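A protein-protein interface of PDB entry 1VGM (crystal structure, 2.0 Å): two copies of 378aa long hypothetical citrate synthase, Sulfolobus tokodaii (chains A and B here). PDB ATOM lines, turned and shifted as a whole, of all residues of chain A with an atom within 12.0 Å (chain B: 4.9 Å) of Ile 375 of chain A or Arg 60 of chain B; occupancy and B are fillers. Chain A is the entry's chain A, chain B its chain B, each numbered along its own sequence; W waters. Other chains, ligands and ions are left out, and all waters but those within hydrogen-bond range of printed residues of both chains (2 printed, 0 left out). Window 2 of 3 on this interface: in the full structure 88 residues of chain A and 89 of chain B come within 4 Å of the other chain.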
ATOM      1  N   GLU A 371       9.093  -9.475  11.139  1.00  0.00           N
ATOM      2  CA  GLU A 371      10.419 -10.045  11.345  1.00  0.00           C
ATOM      3  C   GLU A 371      10.819 -10.936  10.175  1.00  0.00           C
ATOM      4  O   GLU A 371       9.934 -11.521   9.533  1.00  0.00           O
ATOM      5  CB  GLU A 371      10.365 -11.136  12.419  1.00  0.00           C
ATOM      6  CG  GLU A 371       9.441 -12.293  12.081  1.00  0.00           C
ATOM      7  CD  GLU A 371       9.676 -13.504  12.961  1.00  0.00           C
ATOM      8  OE1 GLU A 371       8.772 -13.854  13.749  1.00  0.00           O
ATOM      9  OE2 GLU A 371      10.767 -14.106  12.867  1.00  0.00           O
ATOM     10  N   PHE A 372      12.093 -10.998   9.885  1.00  0.00           N
ATOM     11  CA  PHE A 372      12.570 -11.807   8.776  1.00  0.00           C
ATOM     12  C   PHE A 372      12.159 -13.265   8.913  1.00  0.00           C
ATOM     13  O   PHE A 372      12.124 -13.803  10.017  1.00  0.00           O
ATOM     14  CB  PHE A 372      14.090 -11.733   8.675  1.00  0.00           C
ATOM     15  CG  PHE A 372      14.647 -12.473   7.496  1.00  0.00           C
ATOM     16  CD1 PHE A 372      15.241 -13.723   7.656  1.00  0.00           C
ATOM     17  CD2 PHE A 372      14.546 -11.935   6.214  1.00  0.00           C
ATOM     18  CE1 PHE A 372      15.743 -14.423   6.553  1.00  0.00           C
ATOM     19  CE2 PHE A 372      15.043 -12.625   5.107  1.00  0.00           C
ATOM     20  CZ  PHE A 372      15.637 -13.875   5.277  1.00  0.00           C
ATOM     21  N   LYS A 373      11.878 -13.902   7.778  1.00  0.00           N
ATOM     22  CA  LYS A 373      11.462 -15.300   7.751  1.00  0.00           C
ATOM     23  C   LYS A 373      12.421 -16.158   6.916  1.00  0.00           C
ATOM     24  O   LYS A 373      12.401 -16.106   5.688  1.00  0.00           O
ATOM     25  CB  LYS A 373      10.043 -15.401   7.182  1.00  0.00           C
ATOM     26  CG  LYS A 373       9.472 -16.809   7.185  1.00  0.00           C
ATOM     27  CD  LYS A 373       7.977 -16.804   6.910  1.00  0.00           C
ATOM     28  CE  LYS A 373       7.195 -16.351   8.129  1.00  0.00           C
ATOM     29  NZ  LYS A 373       5.771 -16.799   8.081  1.00  0.00           N
ATOM     30  N   PRO A 374      13.270 -16.968   7.578  1.00  0.00           N
ATOM     31  CA  PRO A 374      14.184 -17.818   6.809  1.00  0.00           C
ATOM     32  C   PRO A 374      13.449 -18.668   5.784  1.00  0.00           C
ATOM     33  O   PRO A 374      12.269 -18.978   5.950  1.00  0.00           O
ATOM     34  CB  PRO A 374      14.877 -18.674   7.875  1.00  0.00           C
ATOM     35  CG  PRO A 374      14.004 -18.595   9.070  1.00  0.00           C
ATOM     36  CD  PRO A 374      13.391 -17.218   9.025  1.00  0.00           C
ATOM     37  N   ILE A 375      14.156 -19.047   4.728  1.00  0.00           N
ATOM     38  CA  ILE A 375      13.521 -19.662   3.574  1.00  0.00           C
ATOM     39  C   ILE A 375      12.863 -21.011   3.907  1.00  0.00           C
ATOM     40  O   ILE A 375      11.868 -21.390   3.294  1.00  0.00           O
ATOM     41  CB  ILE A 375      14.553 -19.828   2.416  1.00  0.00           C
ATOM     42  CG1 ILE A 375      13.826 -20.111   1.101  1.00  0.00           C
ATOM     43  CG2 ILE A 375      15.559 -20.934   2.750  1.00  0.00           C
ATOM     44  CD1 ILE A 375      14.715 -19.978  -0.115  1.00  0.00           C
ATOM     45  N   GLU A 376      13.398 -21.727   4.891  1.00  0.00           N
ATOM     46  CA  GLU A 376      12.861 -23.041   5.243  1.00  0.00           C
ATOM     47  C   GLU A 376      11.511 -22.943   5.944  1.00  0.00           C
ATOM     48  O   GLU A 376      10.791 -23.929   6.060  1.00  0.00           O
ATOM     49  CB  GLU A 376      13.841 -23.806   6.144  1.00  0.00           C
ATOM     50  CG  GLU A 376      15.081 -24.333   5.416  1.00  0.00           C
ATOM     51  CD  GLU A 376      15.693 -25.561   6.087  1.00  0.00           C
ATOM     52  OE1 GLU A 376      16.571 -26.202   5.471  1.00  0.00           O
ATOM     53  OE2 GLU A 376      15.296 -25.886   7.229  1.00  0.00           O
ATOM     54  N   LEU A 377      11.174 -21.752   6.417  1.00  0.00           N
ATOM     55  CA  LEU A 377       9.910 -21.551   7.108  1.00  0.00           C
ATOM     56  C   LEU A 377       8.839 -20.950   6.195  1.00  0.00           C
ATOM     57  O   LEU A 377       7.734 -20.652   6.648  1.00  0.00           O
ATOM     58  CB  LEU A 377      10.117 -20.642   8.322  1.00  0.00           C
ATOM     59  CG  LEU A 377      10.598 -21.283   9.627  1.00  0.00           C
ATOM     60  CD1 LEU A 377      11.831 -22.142   9.389  1.00  0.00           C
ATOM     61  CD2 LEU A 377      10.909 -20.178  10.624  1.00  0.00           C
ATOM     62  N   ARG A 378       9.165 -20.769   4.915  1.00  0.00           N
ATOM     63  CA  ARG A 378       8.270 -20.066   3.996  1.00  0.00           C
ATOM     64  C   ARG A 378       7.283 -20.991   3.303  1.00  0.00           C
ATOM     65  O   ARG A 378       6.212 -20.495   2.892  1.00  0.00           O
ATOM     66  CB  ARG A 378       9.076 -19.316   2.936  1.00  0.00           C
ATOM     67  CG  ARG A 378       9.864 -18.162   3.496  1.00  0.00           C
ATOM     68  CD  ARG A 378      10.800 -17.567   2.466  1.00  0.00           C
ATOM     69  NE  ARG A 378      11.797 -16.733   3.124  1.00  0.00           N
ATOM     70  CZ  ARG A 378      12.903 -16.280   2.540  1.00  0.00           C
ATOM     71  NH1 ARG A 378      13.071 -16.416   1.228  1.00  0.00           N
ATOM     72  NH2 ARG A 378      13.846 -15.700   3.277  1.00  0.00           N
ATOM     73  OXT ARG A 378       7.595 -22.192   3.168  1.00  0.00           O
ATOM     74  N   GLU B  47      15.866 -13.068  -4.105  1.00  0.00           N
ATOM     75  CA  GLU B  47      14.720 -13.167  -3.211  1.00  0.00           C
ATOM     76  C   GLU B  47      13.985 -11.828  -3.149  1.00  0.00           C
ATOM     77  O   GLU B  47      12.757 -11.787  -3.058  1.00  0.00           O
ATOM     78  CB  GLU B  47      15.169 -13.599  -1.809  1.00  0.00           C
ATOM     79  CG  GLU B  47      15.728 -15.021  -1.758  1.00  0.00           C
ATOM     80  CD  GLU B  47      16.420 -15.340  -0.442  1.00  0.00           C
ATOM     81  OE1 GLU B  47      15.776 -15.937   0.449  1.00  0.00           O
ATOM     82  OE2 GLU B  47      17.609 -14.996  -0.297  1.00  0.00           O
ATOM     83  N   PRO B  58      10.307 -15.703  -1.315  1.00  0.00           N
ATOM     84  CA  PRO B  58      10.053 -16.976  -2.002  1.00  0.00           C
ATOM     85  C   PRO B  58      10.490 -18.203  -1.204  1.00  0.00           C
ATOM     86  O   PRO B  58      11.536 -18.187  -0.565  1.00  0.00           O
ATOM     87  CB  PRO B  58      10.850 -16.839  -3.288  1.00  0.00           C
ATOM     88  CG  PRO B  58      12.032 -16.015  -2.871  1.00  0.00           C
ATOM     89  CD  PRO B  58      11.498 -15.021  -1.856  1.00  0.00           C
ATOM     90  N   ASN B  59       9.713 -19.280  -1.265  1.00  0.00           N
ATOM     91  CA  ASN B  59      10.215 -20.565  -0.790  1.00  0.00           C
ATOM     92  C   ASN B  59      11.261 -21.069  -1.776  1.00  0.00           C
ATOM     93  O   ASN B  59      11.549 -20.407  -2.778  1.00  0.00           O
ATOM     94  CB  ASN B  59       9.068 -21.588  -0.625  1.00  0.00           C
ATOM     95  CG  ASN B  59       8.313 -21.860  -1.924  1.00  0.00           C
ATOM     96  OD1 ASN B  59       8.897 -21.879  -3.007  1.00  0.00           O
ATOM     97  ND2 ASN B  59       7.007 -22.087  -1.810  1.00  0.00           N
ATOM     98  N   ARG B  60      11.852 -22.221  -1.476  1.00  0.00           N
ATOM     99  CA  ARG B  60      12.941 -22.750  -2.285  1.00  0.00           C
ATOM    100  C   ARG B  60      12.515 -22.847  -3.741  1.00  0.00           C
ATOM    101  O   ARG B  60      13.220 -22.388  -4.643  1.00  0.00           O
ATOM    102  CB  ARG B  60      13.358 -24.138  -1.789  1.00  0.00           C
ATOM    103  CG  ARG B  60      14.460 -24.774  -2.632  1.00  0.00           C
ATOM    104  CD  ARG B  60      15.710 -23.889  -2.656  1.00  0.00           C
ATOM    105  NE  ARG B  60      16.258 -23.658  -1.318  1.00  0.00           N
ATOM    106  CZ  ARG B  60      17.260 -22.825  -1.048  1.00  0.00           C
ATOM    107  NH1 ARG B  60      17.724 -22.718   0.193  1.00  0.00           N
ATOM    108  NH2 ARG B  60      17.797 -22.095  -2.018  1.00  0.00           N
ATOM    109  N   GLN B  61      11.353 -23.451  -3.957  1.00  0.00           N
ATOM    110  CA  GLN B  61      10.866 -23.741  -5.297  1.00  0.00           C
ATOM    111  C   GLN B  61      10.615 -22.457  -6.094  1.00  0.00           C
ATOM    112  O   GLN B  61      11.021 -22.351  -7.249  1.00  0.00           O
ATOM    113  CB  GLN B  61       9.586 -24.579  -5.195  1.00  0.00           C
ATOM    114  CG  GLN B  61       8.696 -24.575  -6.424  1.00  0.00           C
ATOM    115  CD  GLN B  61       7.224 -24.647  -6.054  1.00  0.00           C
ATOM    116  OE1 GLN B  61       6.745 -25.677  -5.570  1.00  0.00           O
ATOM    117  NE2 GLN B  61       6.501 -23.547  -6.267  1.00  0.00           N
ATOM    118  N   GLN B  62       9.953 -21.482  -5.478  1.00  0.00           N
ATOM    119  CA  GLN B  62       9.742 -20.188  -6.127  1.00  0.00           C
ATOM    120  C   GLN B  62      11.072 -19.479  -6.410  1.00  0.00           C
ATOM    121  O   GLN B  62      11.266 -18.910  -7.479  1.00  0.00           O
ATOM    122  CB  GLN B  62       8.862 -19.291  -5.257  1.00  0.00           C
ATOM    123  CG  GLN B  62       7.480 -19.845  -4.977  1.00  0.00           C
ATOM    124  CD  GLN B  62       6.774 -19.069  -3.883  1.00  0.00           C
ATOM    125  OE1 GLN B  62       7.399 -18.630  -2.917  1.00  0.00           O
ATOM    126  NE2 GLN B  62       5.469 -18.892  -4.030  1.00  0.00           N
ATOM    127  N   LEU B  63      11.987 -19.519  -5.446  1.00  0.00           N
ATOM    128  CA  LEU B  63      13.309 -18.937  -5.629  1.00  0.00           C
ATOM    129  C   LEU B  63      14.019 -19.583  -6.813  1.00  0.00           C
ATOM    130  O   LEU B  63      14.657 -18.901  -7.619  1.00  0.00           O
ATOM    131  CB  LEU B  63      14.154 -19.112  -4.360  1.00  0.00           C
ATOM    132  CG  LEU B  63      15.593 -18.603  -4.460  1.00  0.00           C
ATOM    133  CD1 LEU B  63      15.581 -17.150  -4.909  1.00  0.00           C
ATOM    134  CD2 LEU B  63      16.309 -18.758  -3.123  1.00  0.00           C
ATOM    135  N   ASN B  64      13.910 -20.902  -6.927  1.00  0.00           N
ATOM    136  CA  ASN B  64      14.551 -21.592  -8.042  1.00  0.00           C
ATOM    137  C   ASN B  64      13.909 -21.234  -9.382  1.00  0.00           C
ATOM    138  O   ASN B  64      14.578 -21.237 -10.415  1.00  0.00           O
ATOM    139  CB  ASN B  64      14.508 -23.107  -7.825  1.00  0.00           C
ATOM    140  CG  ASN B  64      15.616 -23.588  -6.908  1.00  0.00           C
ATOM    141  OD1 ASN B  64      16.725 -23.060  -6.939  1.00  0.00           O
ATOM    142  ND2 ASN B  64      15.323 -24.587  -6.088  1.00  0.00           N
ATOM    143  N   LYS B  67      15.470 -17.830 -10.415  1.00  0.00           N
ATOM    144  CA  LYS B  67      16.828 -18.025 -10.924  1.00  0.00           C
ATOM    145  C   LYS B  67      16.809 -18.639 -12.318  1.00  0.00           C
ATOM    146  O   LYS B  67      17.620 -18.280 -13.171  1.00  0.00           O
ATOM    147  CB  LYS B  67      17.630 -18.923  -9.972  1.00  0.00           C
ATOM    148  CG  LYS B  67      18.052 -18.225  -8.696  1.00  0.00           C
ATOM    149  CD  LYS B  67      18.643 -19.198  -7.693  1.00  0.00           C
ATOM    150  CE  LYS B  67      18.850 -18.511  -6.351  1.00  0.00           C
ATOM    151  NZ  LYS B  67      19.580 -19.372  -5.380  1.00  0.00           N
HETATM  152  O   HOH W   1      17.073 -15.981   2.872  1.00  0.00           O
HETATM  153  O   HOH W   2      11.510 -23.290   1.254  1.00  0.00           O
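NH1 of Arg 378 of chain A is in salt-bridge range of OE1 of Glu 47 of chain B, 2.9 Å away.
The backbone carbonyl oxygen (O) of Pro 58 of chain B sits at hydrogen-bond distance from the guanidinium group (NH1) of Arg 378 of chain A, 3.0 Å away.
N of Gln 62 of chain B sits at hydrogen-bond distance from OD1 of Asn 59 of chain B (2.7 Å).
The backbone carbonyl oxygen of Arg 60 of chain B sits at hydrogen-bond distance from the side-chain amide nitrogen of Asn 64 of chain B.
The side-chain amide oxygen of Asn 59 of chain B sits at hydrogen-bond distance from the backbone NH of Gln 61 of chain B.
O of Lys 373 of chain A lies within hydrogen-bond range of NE of Arg 378 of chain A.
Among the printed residues, merely in contact across the chains: Ile 375 of chain A with Pro 58 of chain B (3.4 Å), Ile 375 of chain A with Leu 63 of chain B (3.6 Å), Ile 375 of chain A with Arg 60 of chain B (3.8 Å) and Ile 375 of chain A with Asn 59 of chain B (3.97 Å).
Of the printed residues of chain B, Arg 378 of chain A touches Glu 47 (2.9 Å) and Pro 58 (3.0 Å).
Of the printed residues of chain A, Glu 47 of chain B touches Arg 378.
Asn 59 of chain B touches just one residue of chain A: Ile 375.
No residue of chain A comes within 4 Å of Gln 62 of chain B.
Leu 63 of chain B touches one residue of chain A.
No residue of chain A comes within 4 Å of Asn 64 of chain B.
The nearest residue of chain B that does not touch Ile 375 of chain A is Glu 47 of chain B (4.2 Å).
Of the 8 printed residues of chain A, 2 touch a printed residue of chain B.
Hydrophobic or aromatic side chains of chain A within 4 Å of the printed part of chain B: Ile 375.
Of the 9 printed residues of chain B, 5 touch a printed residue of chain A.
Printed residues of chain B that touch a printed residue of chain A: Glu 47, Pro 58, Asn 59, Arg 60 and Leu 63.
Hydrophobic or aromatic side chains of chain B within 4 Å of the printed part of chain A: Pro 58 and Leu 63.
No position is printed for both chains.
Water W1 lies within hydrogen-bond range of the side-chain carboxylate (OE1) of Glu 47 of chain B (2.7 Å) and the guanidinium group (NH2) of Arg 378 of chain A (3.3 Å).
Water W2 bridges the backbone carbonyl oxygen (O) of Ile 375 of chain A (2.8 Å) and the backbone NH (N) of Arg 60 of chain B (3.0 Å).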
